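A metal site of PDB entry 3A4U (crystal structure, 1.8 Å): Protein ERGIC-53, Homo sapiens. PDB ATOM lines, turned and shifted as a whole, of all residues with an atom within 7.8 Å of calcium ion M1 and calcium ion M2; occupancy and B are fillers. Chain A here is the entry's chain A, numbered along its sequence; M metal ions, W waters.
Within 4 Å of calcium ion M2: Asp 122, Phe 124, Asn 126 and Asp 151.
Along chain A the residues within 4 Å of calcium ion M2 span positions 122 to 151.
The nearest printed residue that does not touch calcium ion M2 is His 148 (4.5 Å).
Within 4 Å of calcium ion M1: Asp 125, Asp 127, Asn 131, Asn 132 and Asp 151.
The nearest printed residue that does not touch calcium ion M1 is Lys 129 (4.3 Å).
The backbone NH of Lys 129 lies within hydrogen-bond range of the side-chain carboxylate of Asp 125 (3.1 Å).
The backbone carbonyl oxygen (O) of Phe 124 sits close to the side-chain amide nitrogen (ND2) of Asn 132.
The backbone NH (N) of Asp 122 lies within hydrogen-bond range of the backbone carbonyl oxygen (O) of Ala 134 (2.8 Å).
The backbone NH (N) of Gly 128 sits close to the side-chain carboxylate (OD1) of Asp 125 (3.3 Å).
ND2 of Asn 132 sits at hydrogen-bond distance from O of Asp 122, at 3.0 Å.
The backbone NH (N) of Lys 130 lies within hydrogen-bond range of the side-chain carboxylate (OD2) of Asp 125.
N of Asp 127 lies within hydrogen-bond range of O of Gln 149, 3.4 Å away.
Calcium ion M1 is bound by the side-chain carboxylate (OD2) of Asp 151 (2.3 Å).
OD1 of Asn 131 binds calcium ion M1 (2.4 Å).
OD1 of Asn 132 binds calcium ion M1 (2.4 Å).
The side-chain carboxylate (OD1) of Asp 125 binds calcium ion M1 (2.4 Å).
Calcium ion M1 is bound by water W2.
Calcium ion M1 is bound by water W4.
The side-chain carboxylate (OD1) of Asp 127 is bound to calcium ion M1 (2.5 Å).
Calcium ion M1 has seven donor atoms within binding distance.
Calcium ion M2 is bound by OD1 of Asp 151 (2.3 Å), OD1 of Asn 126 (2.3 Å), O of Phe 124 (2.3 Å), water W1 (2.4 Å), OD1 of Asp 122 (2.4 Å), water W3 (2.5 Å) and OD2 of Asp 122 (2.5 Å).
Calcium ion M2 has seven donor atoms within binding distance.
Water W4 lies within hydrogen-bond range of the backbone carbonyl oxygen (O) of Asn 131 (3.1 Å) and the side-chain amide nitrogen (ND2) of Asn 132 (3.2 Å).
Water W2 bridges the side-chain carboxylate of Asp 127 and the side-chain amide nitrogen of Asn 131.
Water W3 lies within hydrogen-bond range of O of His 148 (2.9 Å) and OH of Tyr 146 (2.9 Å).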
ATOM      1  N   GLY A  89      16.846  18.026 -20.287  1.00  0.00           N
ATOM      2  CA  GLY A  89      16.790  19.026 -19.216  1.00  0.00           C
ATOM      3  C   GLY A  89      17.857  18.772 -18.170  1.00  0.00           C
ATOM      4  O   GLY A  89      18.633  17.825 -18.292  1.00  0.00           O
ATOM      5  N   ALA A  90      17.877  19.623 -17.146  1.00  0.00           N
ATOM      6  CA  ALA A  90      18.823  19.511 -16.035  1.00  0.00           C
ATOM      7  C   ALA A  90      18.319  20.321 -14.837  1.00  0.00           C
ATOM      8  O   ALA A  90      17.507  21.236 -15.015  1.00  0.00           O
ATOM      9  CB  ALA A  90      20.219  19.994 -16.450  1.00  0.00           C
ATOM     10  N   ASP A  91      18.773  19.994 -13.629  1.00  0.00           N
ATOM     11  CA  ASP A  91      19.619  18.837 -13.354  1.00  0.00           C
ATOM     12  C   ASP A  91      18.830  17.673 -12.785  1.00  0.00           C
ATOM     13  O   ASP A  91      19.169  16.508 -13.008  1.00  0.00           O
ATOM     14  CB  ASP A  91      20.722  19.211 -12.374  1.00  0.00           C
ATOM     15  CG  ASP A  91      21.998  19.560 -13.078  1.00  0.00           C
ATOM     16  OD1 ASP A  91      22.311  20.763 -13.163  1.00  0.00           O
ATOM     17  OD2 ASP A  91      22.683  18.619 -13.577  1.00  0.00           O
ATOM     18  N   GLY A  92      17.791  18.003 -12.028  1.00  0.00           N
ATOM     19  CA  GLY A  92      16.917  17.000 -11.463  1.00  0.00           C
ATOM     20  C   GLY A  92      16.428  17.361 -10.077  1.00  0.00           C
ATOM     21  O   GLY A  92      16.731  18.440  -9.553  1.00  0.00           O
ATOM     22  N   PHE A 108      21.897  18.119  -6.075  1.00  0.00           N
ATOM     23  CA  PHE A 108      20.543  18.495  -6.482  1.00  0.00           C
ATOM     24  C   PHE A 108      19.971  19.577  -5.564  1.00  0.00           C
ATOM     25  O   PHE A 108      18.821  19.512  -5.130  1.00  0.00           O
ATOM     26  CB  PHE A 108      19.634  17.248  -6.567  1.00  0.00           C
ATOM     27  CG  PHE A 108      20.083  16.261  -7.617  1.00  0.00           C
ATOM     28  CD1 PHE A 108      19.740  16.444  -8.961  1.00  0.00           C
ATOM     29  CD2 PHE A 108      20.859  15.160  -7.259  1.00  0.00           C
ATOM     30  CE1 PHE A 108      20.182  15.547  -9.937  1.00  0.00           C
ATOM     31  CE2 PHE A 108      21.300  14.249  -8.234  1.00  0.00           C
ATOM     32  CZ  PHE A 108      20.958  14.447  -9.568  1.00  0.00           C
ATOM     33  N   PHE A 121      16.168  11.978  -8.896  1.00  0.00           N
ATOM     34  CA  PHE A 121      15.529  11.988 -10.205  1.00  0.00           C
ATOM     35  C   PHE A 121      16.435  12.804 -11.108  1.00  0.00           C
ATOM     36  O   PHE A 121      16.344  14.027 -11.196  1.00  0.00           O
ATOM     37  CB  PHE A 121      14.104  12.565 -10.086  1.00  0.00           C
ATOM     38  CG  PHE A 121      13.218  11.723  -9.220  1.00  0.00           C
ATOM     39  CD1 PHE A 121      12.240  10.917  -9.797  1.00  0.00           C
ATOM     40  CD2 PHE A 121      13.400  11.685  -7.844  1.00  0.00           C
ATOM     41  CE1 PHE A 121      11.436  10.116  -9.010  1.00  0.00           C
ATOM     42  CE2 PHE A 121      12.600  10.877  -7.036  1.00  0.00           C
ATOM     43  CZ  PHE A 121      11.611  10.087  -7.624  1.00  0.00           C
ATOM     44  N   ASP A 122      17.352  12.090 -11.748  1.00  0.00           N
ATOM     45  CA  ASP A 122      18.475  12.703 -12.427  1.00  0.00           C
ATOM     46  C   ASP A 122      18.203  12.811 -13.923  1.00  0.00           C
ATOM     47  O   ASP A 122      18.297  11.824 -14.661  1.00  0.00           O
ATOM     48  CB  ASP A 122      19.735  11.861 -12.168  1.00  0.00           C
ATOM     49  CG  ASP A 122      20.990  12.497 -12.741  1.00  0.00           C
ATOM     50  OD1 ASP A 122      20.876  13.411 -13.584  1.00  0.00           O
ATOM     51  OD2 ASP A 122      22.103  12.075 -12.335  1.00  0.00           O
ATOM     52  N   SER A 123      17.913  14.034 -14.373  1.00  0.00           N
ATOM     53  CA  SER A 123      17.532  14.283 -15.772  1.00  0.00           C
ATOM     54  C   SER A 123      18.708  14.304 -16.724  1.00  0.00           C
ATOM     55  O   SER A 123      18.537  14.014 -17.919  1.00  0.00           O
ATOM     56  CB  SER A 123      16.832  15.643 -15.891  1.00  0.00           C
ATOM     57  OG  SER A 123      15.716  15.710 -15.032  1.00  0.00           O
ATOM     58  N   PHE A 124      19.875  14.665 -16.221  1.00  0.00           N
ATOM     59  CA  PHE A 124      21.004  14.960 -17.101  1.00  0.00           C
ATOM     60  C   PHE A 124      22.120  13.913 -17.028  1.00  0.00           C
ATOM     61  O   PHE A 124      22.648  13.590 -15.967  1.00  0.00           O
ATOM     62  CB  PHE A 124      21.552  16.365 -16.834  1.00  0.00           C
ATOM     63  CG  PHE A 124      22.579  16.810 -17.829  1.00  0.00           C
ATOM     64  CD1 PHE A 124      22.201  17.317 -19.073  1.00  0.00           C
ATOM     65  CD2 PHE A 124      23.940  16.706 -17.528  1.00  0.00           C
ATOM     66  CE1 PHE A 124      23.163  17.732 -19.999  1.00  0.00           C
ATOM     67  CE2 PHE A 124      24.900  17.107 -18.454  1.00  0.00           C
ATOM     68  CZ  PHE A 124      24.516  17.623 -19.689  1.00  0.00           C
ATOM     69  N   ASP A 125      22.438  13.394 -18.204  1.00  0.00           N
ATOM     70  CA  ASP A 125      23.392  12.298 -18.398  1.00  0.00           C
ATOM     71  C   ASP A 125      24.838  12.827 -18.352  1.00  0.00           C
ATOM     72  O   ASP A 125      25.455  13.068 -19.386  1.00  0.00           O
ATOM     73  CB  ASP A 125      23.056  11.665 -19.753  1.00  0.00           C
ATOM     74  CG  ASP A 125      23.876  10.415 -20.075  1.00  0.00           C
ATOM     75  OD1 ASP A 125      24.364   9.719 -19.165  1.00  0.00           O
ATOM     76  OD2 ASP A 125      24.010  10.155 -21.287  1.00  0.00           O
ATOM     77  N   ASN A 126      25.366  13.012 -17.141  1.00  0.00           N
ATOM     78  CA  ASN A 126      26.709  13.576 -16.962  1.00  0.00           C
ATOM     79  C   ASN A 126      27.847  12.703 -17.470  1.00  0.00           C
ATOM     80  O   ASN A 126      28.922  13.226 -17.805  1.00  0.00           O
ATOM     81  CB  ASN A 126      26.961  13.954 -15.506  1.00  0.00           C
ATOM     82  CG  ASN A 126      26.173  15.161 -15.089  1.00  0.00           C
ATOM     83  OD1 ASN A 126      25.067  15.038 -14.569  1.00  0.00           O
ATOM     84  ND2 ASN A 126      26.725  16.352 -15.351  1.00  0.00           N
ATOM     85  N   ASP A 127      27.627  11.395 -17.504  1.00  0.00           N
ATOM     86  CA  ASP A 127      28.653  10.453 -17.965  1.00  0.00           C
ATOM     87  C   ASP A 127      28.475   9.994 -19.421  1.00  0.00           C
ATOM     88  O   ASP A 127      29.284   9.222 -19.934  1.00  0.00           O
ATOM     89  CB  ASP A 127      28.809   9.268 -17.003  1.00  0.00           C
ATOM     90  CG  ASP A 127      27.514   8.490 -16.775  1.00  0.00           C
ATOM     91  OD1 ASP A 127      26.460   8.837 -17.374  1.00  0.00           O
ATOM     92  OD2 ASP A 127      27.545   7.520 -15.993  1.00  0.00           O
ATOM     93  N   GLY A 128      27.423  10.487 -20.079  1.00  0.00           N
ATOM     94  CA  GLY A 128      27.167  10.162 -21.488  1.00  0.00           C
ATOM     95  C   GLY A 128      26.883   8.693 -21.757  1.00  0.00           C
ATOM     96  O   GLY A 128      27.249   8.159 -22.809  1.00  0.00           O
ATOM     97  N   LYS A 129      26.237   8.029 -20.809  1.00  0.00           N
ATOM     98  CA  LYS A 129      25.948   6.598 -20.910  1.00  0.00           C
ATOM     99  C   LYS A 129      24.551   6.307 -21.469  1.00  0.00           C
ATOM    100  O   LYS A 129      24.106   5.160 -21.465  1.00  0.00           O
ATOM    101  CB  LYS A 129      26.152   5.906 -19.563  1.00  0.00           C
ATOM    102  CG  LYS A 129      27.612   5.804 -19.117  1.00  0.00           C
ATOM    103  CD  LYS A 129      28.434   4.970 -20.097  1.00  0.00           C
ATOM    104  CE  LYS A 129      29.922   5.029 -19.769  1.00  0.00           C
ATOM    105  NZ  LYS A 129      30.727   4.434 -20.874  1.00  0.00           N
ATOM    106  N   LYS A 130      23.883   7.366 -21.940  1.00  0.00           N
ATOM    107  CA  LYS A 130      22.582   7.263 -22.615  1.00  0.00           C
ATOM    108  C   LYS A 130      21.541   6.541 -21.755  1.00  0.00           C
ATOM    109  O   LYS A 130      20.713   5.769 -22.256  1.00  0.00           O
ATOM    110  CB  LYS A 130      22.754   6.575 -23.980  1.00  0.00           C
ATOM    111  CG  LYS A 130      23.531   7.381 -24.999  1.00  0.00           C
ATOM    112  CD  LYS A 130      23.785   6.552 -26.260  1.00  0.00           C
ATOM    113  CE  LYS A 130      24.032   7.427 -27.473  1.00  0.00           C
ATOM    114  NZ  LYS A 130      22.755   7.902 -28.102  1.00  0.00           N
ATOM    115  N   ASN A 131      21.603   6.808 -20.454  1.00  0.00           N
ATOM    116  CA  ASN A 131      20.748   6.139 -19.487  1.00  0.00           C
ATOM    117  C   ASN A 131      20.091   7.134 -18.538  1.00  0.00           C
ATOM    118  O   ASN A 131      20.007   6.902 -17.325  1.00  0.00           O
ATOM    119  CB  ASN A 131      21.538   5.080 -18.699  1.00  0.00           C
ATOM    120  CG  ASN A 131      22.743   5.670 -17.967  1.00  0.00           C
ATOM    121  OD1 ASN A 131      23.199   6.772 -18.259  1.00  0.00           O
ATOM    122  ND2 ASN A 131      23.277   4.913 -17.010  1.00  0.00           N
ATOM    123  N   ASN A 132      19.647   8.264 -19.111  1.00  0.00           N
ATOM    124  CA  ASN A 132      18.878   9.278 -18.391  1.00  0.00           C
ATOM    125  C   ASN A 132      17.655   9.700 -19.204  1.00  0.00           C
ATOM    126  O   ASN A 132      17.642   9.516 -20.428  1.00  0.00           O
ATOM    127  CB  ASN A 132      19.730  10.514 -18.097  1.00  0.00           C
ATOM    128  CG  ASN A 132      20.884  10.214 -17.175  1.00  0.00           C
ATOM    129  OD1 ASN A 132      21.854   9.576 -17.576  1.00  0.00           O
ATOM    130  ND2 ASN A 132      20.797  10.677 -15.933  1.00  0.00           N
ATOM    131  N   PRO A 133      16.621  10.253 -18.530  1.00  0.00           N
ATOM    132  CA  PRO A 133      16.497  10.418 -17.082  1.00  0.00           C
ATOM    133  C   PRO A 133      16.474   9.089 -16.312  1.00  0.00           C
ATOM    134  O   PRO A 133      15.965   8.082 -16.811  1.00  0.00           O
ATOM    135  CB  PRO A 133      15.162  11.156 -16.927  1.00  0.00           C
ATOM    136  CG  PRO A 133      14.985  11.862 -18.223  1.00  0.00           C
ATOM    137  CD  PRO A 133      15.472  10.858 -19.220  1.00  0.00           C
ATOM    138  N   ALA A 134      17.053   9.110 -15.118  1.00  0.00           N
ATOM    139  CA  ALA A 134      17.148   7.940 -14.280  1.00  0.00           C
ATOM    140  C   ALA A 134      16.718   8.273 -12.859  1.00  0.00           C
ATOM    141  O   ALA A 134      16.740   9.442 -12.456  1.00  0.00           O
ATOM    142  CB  ALA A 134      18.569   7.383 -14.301  1.00  0.00           C
ATOM    143  N   VAL A 136      17.757   7.188  -9.086  1.00  0.00           N
ATOM    144  CA  VAL A 136      18.940   6.574  -8.484  1.00  0.00           C
ATOM    145  C   VAL A 136      18.862   6.692  -6.971  1.00  0.00           C
ATOM    146  O   VAL A 136      18.709   7.792  -6.433  1.00  0.00           O
ATOM    147  CB  VAL A 136      20.240   7.250  -9.006  1.00  0.00           C
ATOM    148  CG1 VAL A 136      21.464   6.517  -8.526  1.00  0.00           C
ATOM    149  CG2 VAL A 136      20.250   7.303 -10.554  1.00  0.00           C
ATOM    150  N   TYR A 146      28.860  12.643  -3.216  1.00  0.00           N
ATOM    151  CA  TYR A 146      28.082  12.256  -4.409  1.00  0.00           C
ATOM    152  C   TYR A 146      28.918  12.412  -5.688  1.00  0.00           C
ATOM    153  O   TYR A 146      29.534  13.453  -5.927  1.00  0.00           O
ATOM    154  CB  TYR A 146      26.796  13.083  -4.488  1.00  0.00           C
ATOM    155  CG  TYR A 146      26.047  12.923  -5.782  1.00  0.00           C
ATOM    156  CD1 TYR A 146      25.522  11.688  -6.158  1.00  0.00           C
ATOM    157  CD2 TYR A 146      25.844  14.021  -6.631  1.00  0.00           C
ATOM    158  CE1 TYR A 146      24.818  11.534  -7.361  1.00  0.00           C
ATOM    159  CE2 TYR A 146      25.148  13.873  -7.824  1.00  0.00           C
ATOM    160  CZ  TYR A 146      24.644  12.643  -8.189  1.00  0.00           C
ATOM    161  OH  TYR A 146      23.963  12.509  -9.371  1.00  0.00           O
ATOM    162  N   ASP A 147      28.931  11.367  -6.517  1.00  0.00           N
ATOM    163  CA  ASP A 147      29.701  11.362  -7.760  1.00  0.00           C
ATOM    164  C   ASP A 147      28.832  11.949  -8.875  1.00  0.00           C
ATOM    165  O   ASP A 147      28.232  11.211  -9.646  1.00  0.00           O
ATOM    166  CB  ASP A 147      30.171   9.945  -8.101  1.00  0.00           C
ATOM    167  CG  ASP A 147      31.124   9.896  -9.291  1.00  0.00           C
ATOM    168  OD1 ASP A 147      31.372  10.929  -9.951  1.00  0.00           O
ATOM    169  OD2 ASP A 147      31.632   8.791  -9.579  1.00  0.00           O
ATOM    170  N   HIS A 148      28.783  13.282  -8.937  1.00  0.00           N
ATOM    171  CA  HIS A 148      27.920  13.991  -9.889  1.00  0.00           C
ATOM    172  C   HIS A 148      28.313  13.691 -11.334  1.00  0.00           C
ATOM    173  O   HIS A 148      27.443  13.471 -12.181  1.00  0.00           O
ATOM    174  CB  HIS A 148      27.916  15.507  -9.598  1.00  0.00           C
ATOM    175  CG  HIS A 148      26.846  16.256 -10.343  1.00  0.00           C
ATOM    176  ND1 HIS A 148      27.044  16.799 -11.588  1.00  0.00           N
ATOM    177  CD2 HIS A 148      25.572  16.568  -9.988  1.00  0.00           C
ATOM    178  CE1 HIS A 148      25.935  17.414 -11.986  1.00  0.00           C
ATOM    179  NE2 HIS A 148      25.023  17.280 -11.034  1.00  0.00           N
ATOM    180  N   GLN A 149      29.609  13.645 -11.603  1.00  0.00           N
ATOM    181  CA  GLN A 149      30.138  13.445 -12.957  1.00  0.00           C
ATOM    182  C   GLN A 149      29.708  12.105 -13.592  1.00  0.00           C
ATOM    183  O   GLN A 149      29.647  11.985 -14.822  1.00  0.00           O
ATOM    184  CB  GLN A 149      31.666  13.588 -12.974  1.00  0.00           C
ATOM    185  CG  GLN A 149      32.154  15.022 -12.722  1.00  0.00           C
ATOM    186  CD  GLN A 149      33.665  15.171 -12.810  1.00  0.00           C
ATOM    187  OE1 GLN A 149      34.417  14.575 -12.022  1.00  0.00           O
ATOM    188  NE2 GLN A 149      34.125  15.995 -13.757  1.00  0.00           N
ATOM    189  N   ASN A 150      29.426  11.115 -12.756  1.00  0.00           N
ATOM    190  CA  ASN A 150      29.011   9.804 -13.221  1.00  0.00           C
ATOM    191  C   ASN A 150      27.574   9.440 -12.826  1.00  0.00           C
ATOM    192  O   ASN A 150      27.210   8.269 -12.785  1.00  0.00           O
ATOM    193  CB  ASN A 150      29.998   8.739 -12.734  1.00  0.00           C
ATOM    194  CG  ASN A 150      31.389   8.935 -13.312  1.00  0.00           C
ATOM    195  OD1 ASN A 150      31.586   8.838 -14.520  1.00  0.00           O
ATOM    196  ND2 ASN A 150      32.359   9.221 -12.445  1.00  0.00           N
ATOM    197  N   ASP A 151      26.769  10.471 -12.529  1.00  0.00           N
ATOM    198  CA  ASP A 151      25.368  10.274 -12.131  1.00  0.00           C
ATOM    199  C   ASP A 151      25.214   9.262 -10.986  1.00  0.00           C
ATOM    200  O   ASP A 151      24.232   8.504 -10.933  1.00  0.00           O
ATOM    201  CB  ASP A 151      24.519   9.833 -13.325  1.00  0.00           C
ATOM    202  CG  ASP A 151      24.495  10.863 -14.441  1.00  0.00           C
ATOM    203  OD1 ASP A 151      24.693  12.066 -14.161  1.00  0.00           O
ATOM    204  OD2 ASP A 151      24.250  10.471 -15.594  1.00  0.00           O
ATOM    205  N   GLY A 152      26.206   9.239 -10.088  1.00  0.00           N
ATOM    206  CA  GLY A 152      26.239   8.345  -8.930  1.00  0.00           C
ATOM    207  C   GLY A 152      26.206   6.861  -9.254  1.00  0.00           C
ATOM    208  O   GLY A 152      25.806   6.059  -8.415  1.00  0.00           O
ATOM    209  N   ALA A 153      26.661   6.494 -10.452  1.00  0.00           N
ATOM    210  CA  ALA A 153      26.465   5.142 -10.983  1.00  0.00           C
ATOM    211  C   ALA A 153      27.038   4.054 -10.085  1.00  0.00           C
ATOM    212  O   ALA A 153      26.369   3.051  -9.830  1.00  0.00           O
ATOM    213  CB  ALA A 153      27.039   5.033 -12.401  1.00  0.00           C
HETATM  214 CA    CA M   1      23.988   8.624 -17.023  1.00  0.00          CA
HETATM  215 CA    CA M   2      23.261  13.818 -13.721  1.00  0.00          CA
HETATM  216  O   HOH W   1      22.200  15.925 -13.342  1.00  0.00           O
HETATM  217  O   HOH W   2      24.964   6.906 -15.544  1.00  0.00           O
HETATM  218  O   HOH W   3      24.662  14.056 -11.723  1.00  0.00           O
HETATM  219  O   HOH W   4      22.286   7.853 -15.393  1.00  0.00           O
